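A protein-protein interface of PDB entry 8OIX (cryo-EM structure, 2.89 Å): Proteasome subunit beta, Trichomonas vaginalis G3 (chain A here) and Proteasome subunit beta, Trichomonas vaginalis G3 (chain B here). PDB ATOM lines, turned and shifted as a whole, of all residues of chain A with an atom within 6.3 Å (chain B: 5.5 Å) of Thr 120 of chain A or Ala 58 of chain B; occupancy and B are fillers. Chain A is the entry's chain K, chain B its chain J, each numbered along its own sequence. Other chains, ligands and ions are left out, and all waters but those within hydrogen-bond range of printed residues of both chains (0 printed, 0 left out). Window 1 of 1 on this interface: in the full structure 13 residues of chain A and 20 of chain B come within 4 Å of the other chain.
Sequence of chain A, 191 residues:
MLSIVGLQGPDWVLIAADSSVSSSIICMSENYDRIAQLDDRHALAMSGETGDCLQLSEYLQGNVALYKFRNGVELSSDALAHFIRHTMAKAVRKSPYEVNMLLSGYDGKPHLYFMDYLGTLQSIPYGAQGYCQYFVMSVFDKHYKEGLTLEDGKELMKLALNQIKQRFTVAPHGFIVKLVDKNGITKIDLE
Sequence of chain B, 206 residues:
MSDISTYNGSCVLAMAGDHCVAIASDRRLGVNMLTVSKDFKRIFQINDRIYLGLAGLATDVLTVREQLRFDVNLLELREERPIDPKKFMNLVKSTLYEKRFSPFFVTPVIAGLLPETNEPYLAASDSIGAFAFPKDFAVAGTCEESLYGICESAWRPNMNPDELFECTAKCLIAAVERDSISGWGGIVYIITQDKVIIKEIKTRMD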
ATOM      1  N   ARG A  85     -19.773  11.423  25.824  1.00  0.00           N
ATOM      2  CA  ARG A  85     -18.330  11.351  25.644  1.00  0.00           C
ATOM      3  C   ARG A  85     -17.729  12.733  25.431  1.00  0.00           C
ATOM      4  O   ARG A  85     -16.659  13.039  25.961  1.00  0.00           O
ATOM      5  CB  ARG A  85     -17.998  10.453  24.457  1.00  0.00           C
ATOM      6  CG  ARG A  85     -16.579   9.964  24.461  1.00  0.00           C
ATOM      7  CD  ARG A  85     -16.034   9.843  23.059  1.00  0.00           C
ATOM      8  NE  ARG A  85     -15.666  11.146  22.519  1.00  0.00           N
ATOM      9  CZ  ARG A  85     -14.560  11.800  22.841  1.00  0.00           C
ATOM     10  NH1 ARG A  85     -13.685  11.300  23.698  1.00  0.00           N
ATOM     11  NH2 ARG A  85     -14.326  12.987  22.290  1.00  0.00           N
ATOM     12  N   MET A  88     -17.682  14.491  28.790  1.00  0.00           N
ATOM     13  CA  MET A  88     -16.606  14.002  29.648  1.00  0.00           C
ATOM     14  C   MET A  88     -15.242  14.449  29.137  1.00  0.00           C
ATOM     15  O   MET A  88     -14.345  14.744  29.932  1.00  0.00           O
ATOM     16  CB  MET A  88     -16.666  12.480  29.756  1.00  0.00           C
ATOM     17  CG  MET A  88     -18.002  11.945  30.230  1.00  0.00           C
ATOM     18  SD  MET A  88     -18.630  12.789  31.687  1.00  0.00           S
ATOM     19  CE  MET A  88     -17.560  12.125  32.953  1.00  0.00           C
ATOM     20  N   PHE A 114     -19.621   1.676  27.586  1.00  0.00           N
ATOM     21  CA  PHE A 114     -18.664   1.855  28.671  1.00  0.00           C
ATOM     22  C   PHE A 114     -18.079   3.256  28.560  1.00  0.00           C
ATOM     23  O   PHE A 114     -17.342   3.549  27.615  1.00  0.00           O
ATOM     24  CB  PHE A 114     -17.576   0.788  28.584  1.00  0.00           C
ATOM     25  CG  PHE A 114     -16.481   0.934  29.605  1.00  0.00           C
ATOM     26  CD1 PHE A 114     -15.400   1.770  29.376  1.00  0.00           C
ATOM     27  CD2 PHE A 114     -16.519   0.209  30.783  1.00  0.00           C
ATOM     28  CE1 PHE A 114     -14.393   1.896  30.309  1.00  0.00           C
ATOM     29  CE2 PHE A 114     -15.512   0.326  31.717  1.00  0.00           C
ATOM     30  CZ  PHE A 114     -14.448   1.174  31.480  1.00  0.00           C
ATOM     31  N   MET A 115     -18.406   4.125  29.510  1.00  0.00           N
ATOM     32  CA  MET A 115     -17.946   5.501  29.527  1.00  0.00           C
ATOM     33  C   MET A 115     -17.190   5.729  30.825  1.00  0.00           C
ATOM     34  O   MET A 115     -17.522   5.131  31.847  1.00  0.00           O
ATOM     35  CB  MET A 115     -19.128   6.462  29.419  1.00  0.00           C
ATOM     36  CG  MET A 115     -20.175   6.013  28.410  1.00  0.00           C
ATOM     37  SD  MET A 115     -21.041   7.380  27.630  1.00  0.00           S
ATOM     38  CE  MET A 115     -19.654   8.252  26.923  1.00  0.00           C
ATOM     39  N   ASP A 116     -16.154   6.555  30.796  1.00  0.00           N
ATOM     40  CA  ASP A 116     -15.422   6.848  32.018  1.00  0.00           C
ATOM     41  C   ASP A 116     -15.217   8.350  32.147  1.00  0.00           C
ATOM     42  O   ASP A 116     -15.491   9.119  31.221  1.00  0.00           O
ATOM     43  CB  ASP A 116     -14.080   6.103  32.084  1.00  0.00           C
ATOM     44  CG  ASP A 116     -13.183   6.398  30.910  1.00  0.00           C
ATOM     45  OD1 ASP A 116     -13.579   7.179  30.021  1.00  0.00           O
ATOM     46  OD2 ASP A 116     -12.065   5.845  30.887  1.00  0.00           O
ATOM     47  N   TYR A 117     -14.753   8.758  33.330  1.00  0.00           N
ATOM     48  CA  TYR A 117     -14.590  10.179  33.621  1.00  0.00           C
ATOM     49  C   TYR A 117     -13.714  10.859  32.581  1.00  0.00           C
ATOM     50  O   TYR A 117     -13.954  12.017  32.217  1.00  0.00           O
ATOM     51  CB  TYR A 117     -14.003  10.364  35.020  1.00  0.00           C
ATOM     52  CG  TYR A 117     -12.558   9.943  35.147  1.00  0.00           C
ATOM     53  CD1 TYR A 117     -12.203   8.603  35.186  1.00  0.00           C
ATOM     54  CD2 TYR A 117     -11.547  10.891  35.227  1.00  0.00           C
ATOM     55  CE1 TYR A 117     -10.882   8.219  35.301  1.00  0.00           C
ATOM     56  CE2 TYR A 117     -10.225  10.517  35.344  1.00  0.00           C
ATOM     57  CZ  TYR A 117      -9.898   9.179  35.382  1.00  0.00           C
ATOM     58  OH  TYR A 117      -8.581   8.801  35.497  1.00  0.00           O
ATOM     59  N   LEU A 118     -12.685  10.162  32.095  1.00  0.00           N
ATOM     60  CA  LEU A 118     -11.852  10.729  31.044  1.00  0.00           C
ATOM     61  C   LEU A 118     -12.653  10.943  29.768  1.00  0.00           C
ATOM     62  O   LEU A 118     -12.561  12.003  29.139  1.00  0.00           O
ATOM     63  CB  LEU A 118     -10.649   9.825  30.784  1.00  0.00           C
ATOM     64  CG  LEU A 118      -9.686   9.588  31.944  1.00  0.00           C
ATOM     65  CD1 LEU A 118      -9.261   8.136  31.991  1.00  0.00           C
ATOM     66  CD2 LEU A 118      -8.478  10.495  31.814  1.00  0.00           C
ATOM     67  N   GLY A 119     -13.490   9.975  29.399  1.00  0.00           N
ATOM     68  CA  GLY A 119     -14.235  10.077  28.161  1.00  0.00           C
ATOM     69  C   GLY A 119     -13.984   8.973  27.154  1.00  0.00           C
ATOM     70  O   GLY A 119     -14.055   9.211  25.947  1.00  0.00           O
ATOM     71  N   THR A 120     -13.651   7.771  27.620  1.00  0.00           N
ATOM     72  CA  THR A 120     -13.509   6.624  26.728  1.00  0.00           C
ATOM     73  C   THR A 120     -14.889   6.029  26.475  1.00  0.00           C
ATOM     74  O   THR A 120     -15.535   5.533  27.402  1.00  0.00           O
ATOM     75  CB  THR A 120     -12.572   5.575  27.319  1.00  0.00           C
ATOM     76  OG1 THR A 120     -13.260   4.832  28.332  1.00  0.00           O
ATOM     77  CG2 THR A 120     -11.341   6.231  27.917  1.00  0.00           C
ATOM     78  N   LEU A 121     -15.347   6.087  25.228  1.00  0.00           N
ATOM     79  CA  LEU A 121     -16.651   5.566  24.835  1.00  0.00           C
ATOM     80  C   LEU A 121     -16.460   4.269  24.064  1.00  0.00           C
ATOM     81  O   LEU A 121     -15.724   4.235  23.074  1.00  0.00           O
ATOM     82  CB  LEU A 121     -17.412   6.581  23.985  1.00  0.00           C
ATOM     83  CG  LEU A 121     -18.692   6.069  23.330  1.00  0.00           C
ATOM     84  CD1 LEU A 121     -19.644   5.567  24.388  1.00  0.00           C
ATOM     85  CD2 LEU A 121     -19.336   7.157  22.505  1.00  0.00           C
ATOM     86  N   GLN A 122     -17.123   3.207  24.516  1.00  0.00           N
ATOM     87  CA  GLN A 122     -17.025   1.912  23.853  1.00  0.00           C
ATOM     88  C   GLN A 122     -18.337   1.163  24.009  1.00  0.00           C
ATOM     89  O   GLN A 122     -18.761   0.891  25.135  1.00  0.00           O
ATOM     90  CB  GLN A 122     -15.877   1.091  24.426  1.00  0.00           C
ATOM     91  CG  GLN A 122     -15.742  -0.297  23.833  1.00  0.00           C
ATOM     92  CD  GLN A 122     -15.589  -0.278  22.329  1.00  0.00           C
ATOM     93  OE1 GLN A 122     -14.883   0.564  21.776  1.00  0.00           O
ATOM     94  NE2 GLN A 122     -16.251  -1.210  21.655  1.00  0.00           N
ATOM     95  N   GLN A 129     -18.387  -0.544  35.774  1.00  0.00           N
ATOM     96  CA  GLN A 129     -17.534   0.494  36.322  1.00  0.00           C
ATOM     97  C   GLN A 129     -17.491   0.341  37.836  1.00  0.00           C
ATOM     98  O   GLN A 129     -18.477  -0.067  38.467  1.00  0.00           O
ATOM     99  CB  GLN A 129     -18.015   1.891  35.934  1.00  0.00           C
ATOM    100  CG  GLN A 129     -18.148   2.101  34.438  1.00  0.00           C
ATOM    101  CD  GLN A 129     -16.855   2.547  33.791  1.00  0.00           C
ATOM    102  OE1 GLN A 129     -15.786   2.471  34.393  1.00  0.00           O
ATOM    103  NE2 GLN A 129     -16.948   3.021  32.557  1.00  0.00           N
ATOM    104  N   TYR B   7      -2.736   4.037  30.778  1.00  0.00           N
ATOM    105  CA  TYR B   7      -4.093   3.704  31.204  1.00  0.00           C
ATOM    106  C   TYR B   7      -4.807   2.845  30.167  1.00  0.00           C
ATOM    107  O   TYR B   7      -5.359   1.788  30.493  1.00  0.00           O
ATOM    108  CB  TYR B   7      -4.872   4.991  31.480  1.00  0.00           C
ATOM    109  CG  TYR B   7      -6.322   4.801  31.853  1.00  0.00           C
ATOM    110  CD1 TYR B   7      -6.691   4.538  33.164  1.00  0.00           C
ATOM    111  CD2 TYR B   7      -7.322   4.910  30.901  1.00  0.00           C
ATOM    112  CE1 TYR B   7      -8.014   4.377  33.510  1.00  0.00           C
ATOM    113  CE2 TYR B   7      -8.647   4.747  31.236  1.00  0.00           C
ATOM    114  CZ  TYR B   7      -8.989   4.482  32.542  1.00  0.00           C
ATOM    115  OH  TYR B   7     -10.312   4.320  32.880  1.00  0.00           O
ATOM    116  N   ASN B   8      -4.805   3.281  28.911  1.00  0.00           N
ATOM    117  CA  ASN B   8      -5.414   2.539  27.808  1.00  0.00           C
ATOM    118  C   ASN B   8      -4.297   1.963  26.948  1.00  0.00           C
ATOM    119  O   ASN B   8      -3.706   2.670  26.128  1.00  0.00           O
ATOM    120  CB  ASN B   8      -6.341   3.429  26.986  1.00  0.00           C
ATOM    121  CG  ASN B   8      -7.596   3.814  27.735  1.00  0.00           C
ATOM    122  OD1 ASN B   8      -7.938   4.991  27.832  1.00  0.00           O
ATOM    123  ND2 ASN B   8      -8.289   2.821  28.274  1.00  0.00           N
ATOM    124  N   LEU B  29      -9.545  -2.412  24.228  1.00  0.00           N
ATOM    125  CA  LEU B  29      -9.779  -1.258  25.088  1.00  0.00           C
ATOM    126  C   LEU B  29      -9.572  -1.773  26.504  1.00  0.00           C
ATOM    127  O   LEU B  29     -10.430  -2.470  27.053  1.00  0.00           O
ATOM    128  CB  LEU B  29     -11.168  -0.657  24.918  1.00  0.00           C
ATOM    129  CG  LEU B  29     -11.437   0.357  26.036  1.00  0.00           C
ATOM    130  CD1 LEU B  29     -10.408   1.478  26.009  1.00  0.00           C
ATOM    131  CD2 LEU B  29     -12.833   0.919  25.979  1.00  0.00           C
ATOM    132  N   PHE B  40     -12.262  -2.340  20.125  1.00  0.00           N
ATOM    133  CA  PHE B  40     -11.936  -0.921  20.167  1.00  0.00           C
ATOM    134  C   PHE B  40     -11.214  -0.529  18.885  1.00  0.00           C
ATOM    135  O   PHE B  40     -10.180  -1.114  18.542  1.00  0.00           O
ATOM    136  CB  PHE B  40     -11.088  -0.587  21.390  1.00  0.00           C
ATOM    137  CG  PHE B  40     -10.883   0.885  21.591  1.00  0.00           C
ATOM    138  CD1 PHE B  40     -11.839   1.648  22.238  1.00  0.00           C
ATOM    139  CD2 PHE B  40      -9.740   1.507  21.135  1.00  0.00           C
ATOM    140  CE1 PHE B  40     -11.656   3.002  22.417  1.00  0.00           C
ATOM    141  CE2 PHE B  40      -9.551   2.860  21.315  1.00  0.00           C
ATOM    142  CZ  PHE B  40     -10.509   3.607  21.952  1.00  0.00           C
ATOM    143  N   ARG B  42      -8.920   1.736  16.925  1.00  0.00           N
ATOM    144  CA  ARG B  42      -7.878   2.750  17.018  1.00  0.00           C
ATOM    145  C   ARG B  42      -7.431   3.273  15.663  1.00  0.00           C
ATOM    146  O   ARG B  42      -6.848   4.360  15.601  1.00  0.00           O
ATOM    147  CB  ARG B  42      -6.659   2.206  17.771  1.00  0.00           C
ATOM    148  CG  ARG B  42      -6.925   1.953  19.236  1.00  0.00           C
ATOM    149  CD  ARG B  42      -5.689   1.507  19.987  1.00  0.00           C
ATOM    150  NE  ARG B  42      -5.979   1.334  21.405  1.00  0.00           N
ATOM    151  CZ  ARG B  42      -6.046   2.325  22.283  1.00  0.00           C
ATOM    152  NH1 ARG B  42      -5.830   3.579  21.927  1.00  0.00           N
ATOM    153  NH2 ARG B  42      -6.335   2.050  23.552  1.00  0.00           N
ATOM    154  N   GLY B  56      -3.018   5.412  22.070  1.00  0.00           N
ATOM    155  CA  GLY B  56      -2.927   6.131  23.329  1.00  0.00           C
ATOM    156  C   GLY B  56      -4.250   6.089  24.072  1.00  0.00           C
ATOM    157  O   GLY B  56      -5.045   5.165  23.894  1.00  0.00           O
ATOM    158  N   LEU B  57      -4.449   7.101  24.911  1.00  0.00           N
ATOM    159  CA  LEU B  57      -5.649   7.196  25.730  1.00  0.00           C
ATOM    160  C   LEU B  57      -6.897   7.145  24.860  1.00  0.00           C
ATOM    161  O   LEU B  57      -7.050   7.944  23.933  1.00  0.00           O
ATOM    162  CB  LEU B  57      -5.618   8.488  26.547  1.00  0.00           C
ATOM    163  CG  LEU B  57      -6.519   8.531  27.779  1.00  0.00           C
ATOM    164  CD1 LEU B  57      -6.030   7.544  28.824  1.00  0.00           C
ATOM    165  CD2 LEU B  57      -6.578   9.933  28.352  1.00  0.00           C
ATOM    166  N   ALA B  58      -7.779   6.188  25.158  1.00  0.00           N
ATOM    167  CA  ALA B  58      -9.013   6.034  24.394  1.00  0.00           C
ATOM    168  C   ALA B  58      -9.807   7.332  24.341  1.00  0.00           C
ATOM    169  O   ALA B  58     -10.361   7.691  23.293  1.00  0.00           O
ATOM    170  CB  ALA B  58      -9.858   4.914  24.994  1.00  0.00           C
ATOM    171  N   THR B  59      -9.885   8.042  25.471  1.00  0.00           N
ATOM    172  CA  THR B  59     -10.474   9.375  25.478  1.00  0.00           C
ATOM    173  C   THR B  59      -9.864  10.246  24.398  1.00  0.00           C
ATOM    174  O   THR B  59     -10.576  10.830  23.574  1.00  0.00           O
ATOM    175  CB  THR B  59     -10.275  10.035  26.837  1.00  0.00           C
ATOM    176  OG1 THR B  59     -11.016   9.323  27.829  1.00  0.00           O
ATOM    177  CG2 THR B  59     -10.714  11.487  26.786  1.00  0.00           C
ATOM    178  N   ASP B  60      -8.537  10.320  24.364  1.00  0.00           N
ATOM    179  CA  ASP B  60      -7.911  11.190  23.389  1.00  0.00           C
ATOM    180  C   ASP B  60      -7.877  10.550  22.015  1.00  0.00           C
ATOM    181  O   ASP B  60      -7.805  11.274  21.025  1.00  0.00           O
ATOM    182  CB  ASP B  60      -6.497  11.575  23.827  1.00  0.00           C
ATOM    183  CG  ASP B  60      -6.475  12.309  25.149  1.00  0.00           C
ATOM    184  OD1 ASP B  60      -7.295  13.232  25.331  1.00  0.00           O
ATOM    185  OD2 ASP B  60      -5.628  11.974  26.000  1.00  0.00           O
ATOM    186  N   VAL B  61      -8.019   9.226  21.925  1.00  0.00           N
ATOM    187  CA  VAL B  61      -8.153   8.608  20.611  1.00  0.00           C
ATOM    188  C   VAL B  61      -9.433   9.090  19.950  1.00  0.00           C
ATOM    189  O   VAL B  61      -9.421   9.577  18.814  1.00  0.00           O
ATOM    190  CB  VAL B  61      -8.137   7.073  20.729  1.00  0.00           C
ATOM    191  CG1 VAL B  61      -8.659   6.441  19.449  1.00  0.00           C
ATOM    192  CG2 VAL B  61      -6.750   6.573  21.033  1.00  0.00           C
ATOM    193  N   LEU B  62     -10.539   9.064  20.694  1.00  0.00           N
ATOM    194  CA  LEU B  62     -11.805   9.510  20.130  1.00  0.00           C
ATOM    195  C   LEU B  62     -11.826  11.022  19.954  1.00  0.00           C
ATOM    196  O   LEU B  62     -12.319  11.522  18.938  1.00  0.00           O
ATOM    197  CB  LEU B  62     -12.964   9.033  21.003  1.00  0.00           C
ATOM    198  CG  LEU B  62     -13.200   7.526  20.890  1.00  0.00           C
ATOM    199  CD1 LEU B  62     -14.273   7.044  21.848  1.00  0.00           C
ATOM    200  CD2 LEU B  62     -13.561   7.162  19.458  1.00  0.00           C
ATOM    201  N   THR B  63     -11.284  11.768  20.920  1.00  0.00           N
ATOM    202  CA  THR B  63     -11.278  13.223  20.812  1.00  0.00           C
ATOM    203  C   THR B  63     -10.464  13.679  19.608  1.00  0.00           C
ATOM    204  O   THR B  63     -10.913  14.523  18.828  1.00  0.00           O
ATOM    205  CB  THR B  63     -10.737  13.846  22.098  1.00  0.00           C
ATOM    206  OG1 THR B  63     -11.477  13.348  23.219  1.00  0.00           O
ATOM    207  CG2 THR B  63     -10.878  15.355  22.048  1.00  0.00           C
ATOM    208  N   VAL B 106      -2.234  10.633  22.970  1.00  0.00           N
ATOM    209  CA  VAL B 106      -2.274   9.709  21.845  1.00  0.00           C
ATOM    210  C   VAL B 106      -1.157  10.060  20.875  1.00  0.00           C
ATOM    211  O   VAL B 106      -0.907  11.235  20.588  1.00  0.00           O
ATOM    212  CB  VAL B 106      -3.637   9.726  21.125  1.00  0.00           C
ATOM    213  CG1 VAL B 106      -4.702   9.179  22.030  1.00  0.00           C
ATOM    214  CG2 VAL B 106      -3.994  11.133  20.682  1.00  0.00           C
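The side-chain hydroxyl (OH) of Tyr 7 of chain B is in hydrogen-bond range of the side-chain carboxylate (OD2) of Asp 116 of chain A (3.1 Å).
The backbone carbonyl oxygen of Thr 59 of chain B lies within hydrogen-bond range of the guanidinium group of Arg 85 of chain A, 3.1 Å away.
O of Leu 118 of chain A lies close to OG1 of Thr 59 of chain B.
The side-chain hydroxyl of Thr 59 of chain B sits at hydrogen-bond distance from the backbone NH of Gly 119 of chain A, at 3.0 Å.
OG1 of Thr 59 of chain B sits at hydrogen-bond distance from N of Thr 120 of chain A (3.1 Å).
NH2 of Arg 85 of chain A lies within hydrogen-bond range of OG1 of Thr 63 of chain B (3.0 Å).
Among the printed residues, merely in contact across the chains: Arg 85 of chain A with Leu 62 of chain B, Asp 116 of chain A with Thr 59 of chain B, Leu 118 of chain A with Tyr 7 of chain B, Leu 118 of chain A with Leu 57 of chain B, Thr 120 of chain A with Asn 8 of chain B, Thr 120 of chain A with Ala 58 of chain B, Leu 121 of chain A with Leu 62 of chain B, Gln 122 of chain A with Leu 29 of chain B and Gln 122 of chain A with Phe 40 of chain B.
N of Ala 58 of chain B sits at hydrogen-bond distance from OD1 of Asn 8 of chain B, at 2.9 Å.
O of Thr 59 of chain B is in hydrogen-bond range of OG1 of Thr 63 of chain B, 2.7 Å away.
The backbone carbonyl oxygen (O) of Phe 114 of chain A lies close to the backbone carbonyl oxygen (O) of Thr 120 of chain A (2.7 Å).
N of Phe 114 of chain A sits at hydrogen-bond distance from O of Gln 122 of chain A, at 2.7 Å.
The backbone NH (N) of Gly 119 of chain A sits at hydrogen-bond distance from the side-chain carboxylate (OD1) of Asp 116 of chain A (2.9 Å).
OD1 of Asp 116 of chain A sits at hydrogen-bond distance from N of Thr 120 of chain A, 2.5 Å away.
Of the 14 printed residues of chain B, 9 touch a printed residue of chain A.
Hydrophobic or aromatic side chains of chain B that line the printed part of chain A: Tyr 7, Leu 29, Phe 40, Leu 57, Ala 58 and Leu 62.
Hydrophobic or aromatic side chains of chain A within 4 Å of the printed part of chain B: Leu 118 and Leu 121.
Among the printed residues, no Asp or Glu carboxylate lies within 4 Å of a Lys or Arg side-chain nitrogen of the other chain.
Of the printed residues of chain B, Thr 120 of chain A touches Asn 8, Ala 58 and Thr 59.
Of the printed residues of chain A, Ala 58 of chain B touches Thr 120.
Of the printed residues of chain B, Asp 116 of chain A touches Tyr 7 (3.1 Å) and Thr 59 (3.996 Å).
Of the printed residues of chain B, Leu 121 of chain A touches Leu 62 (3.4 Å).
Of the printed residues of chain A, Asn 8 of chain B touches Thr 120.
Val 106 of chain B touches none of the printed residues of chain A.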
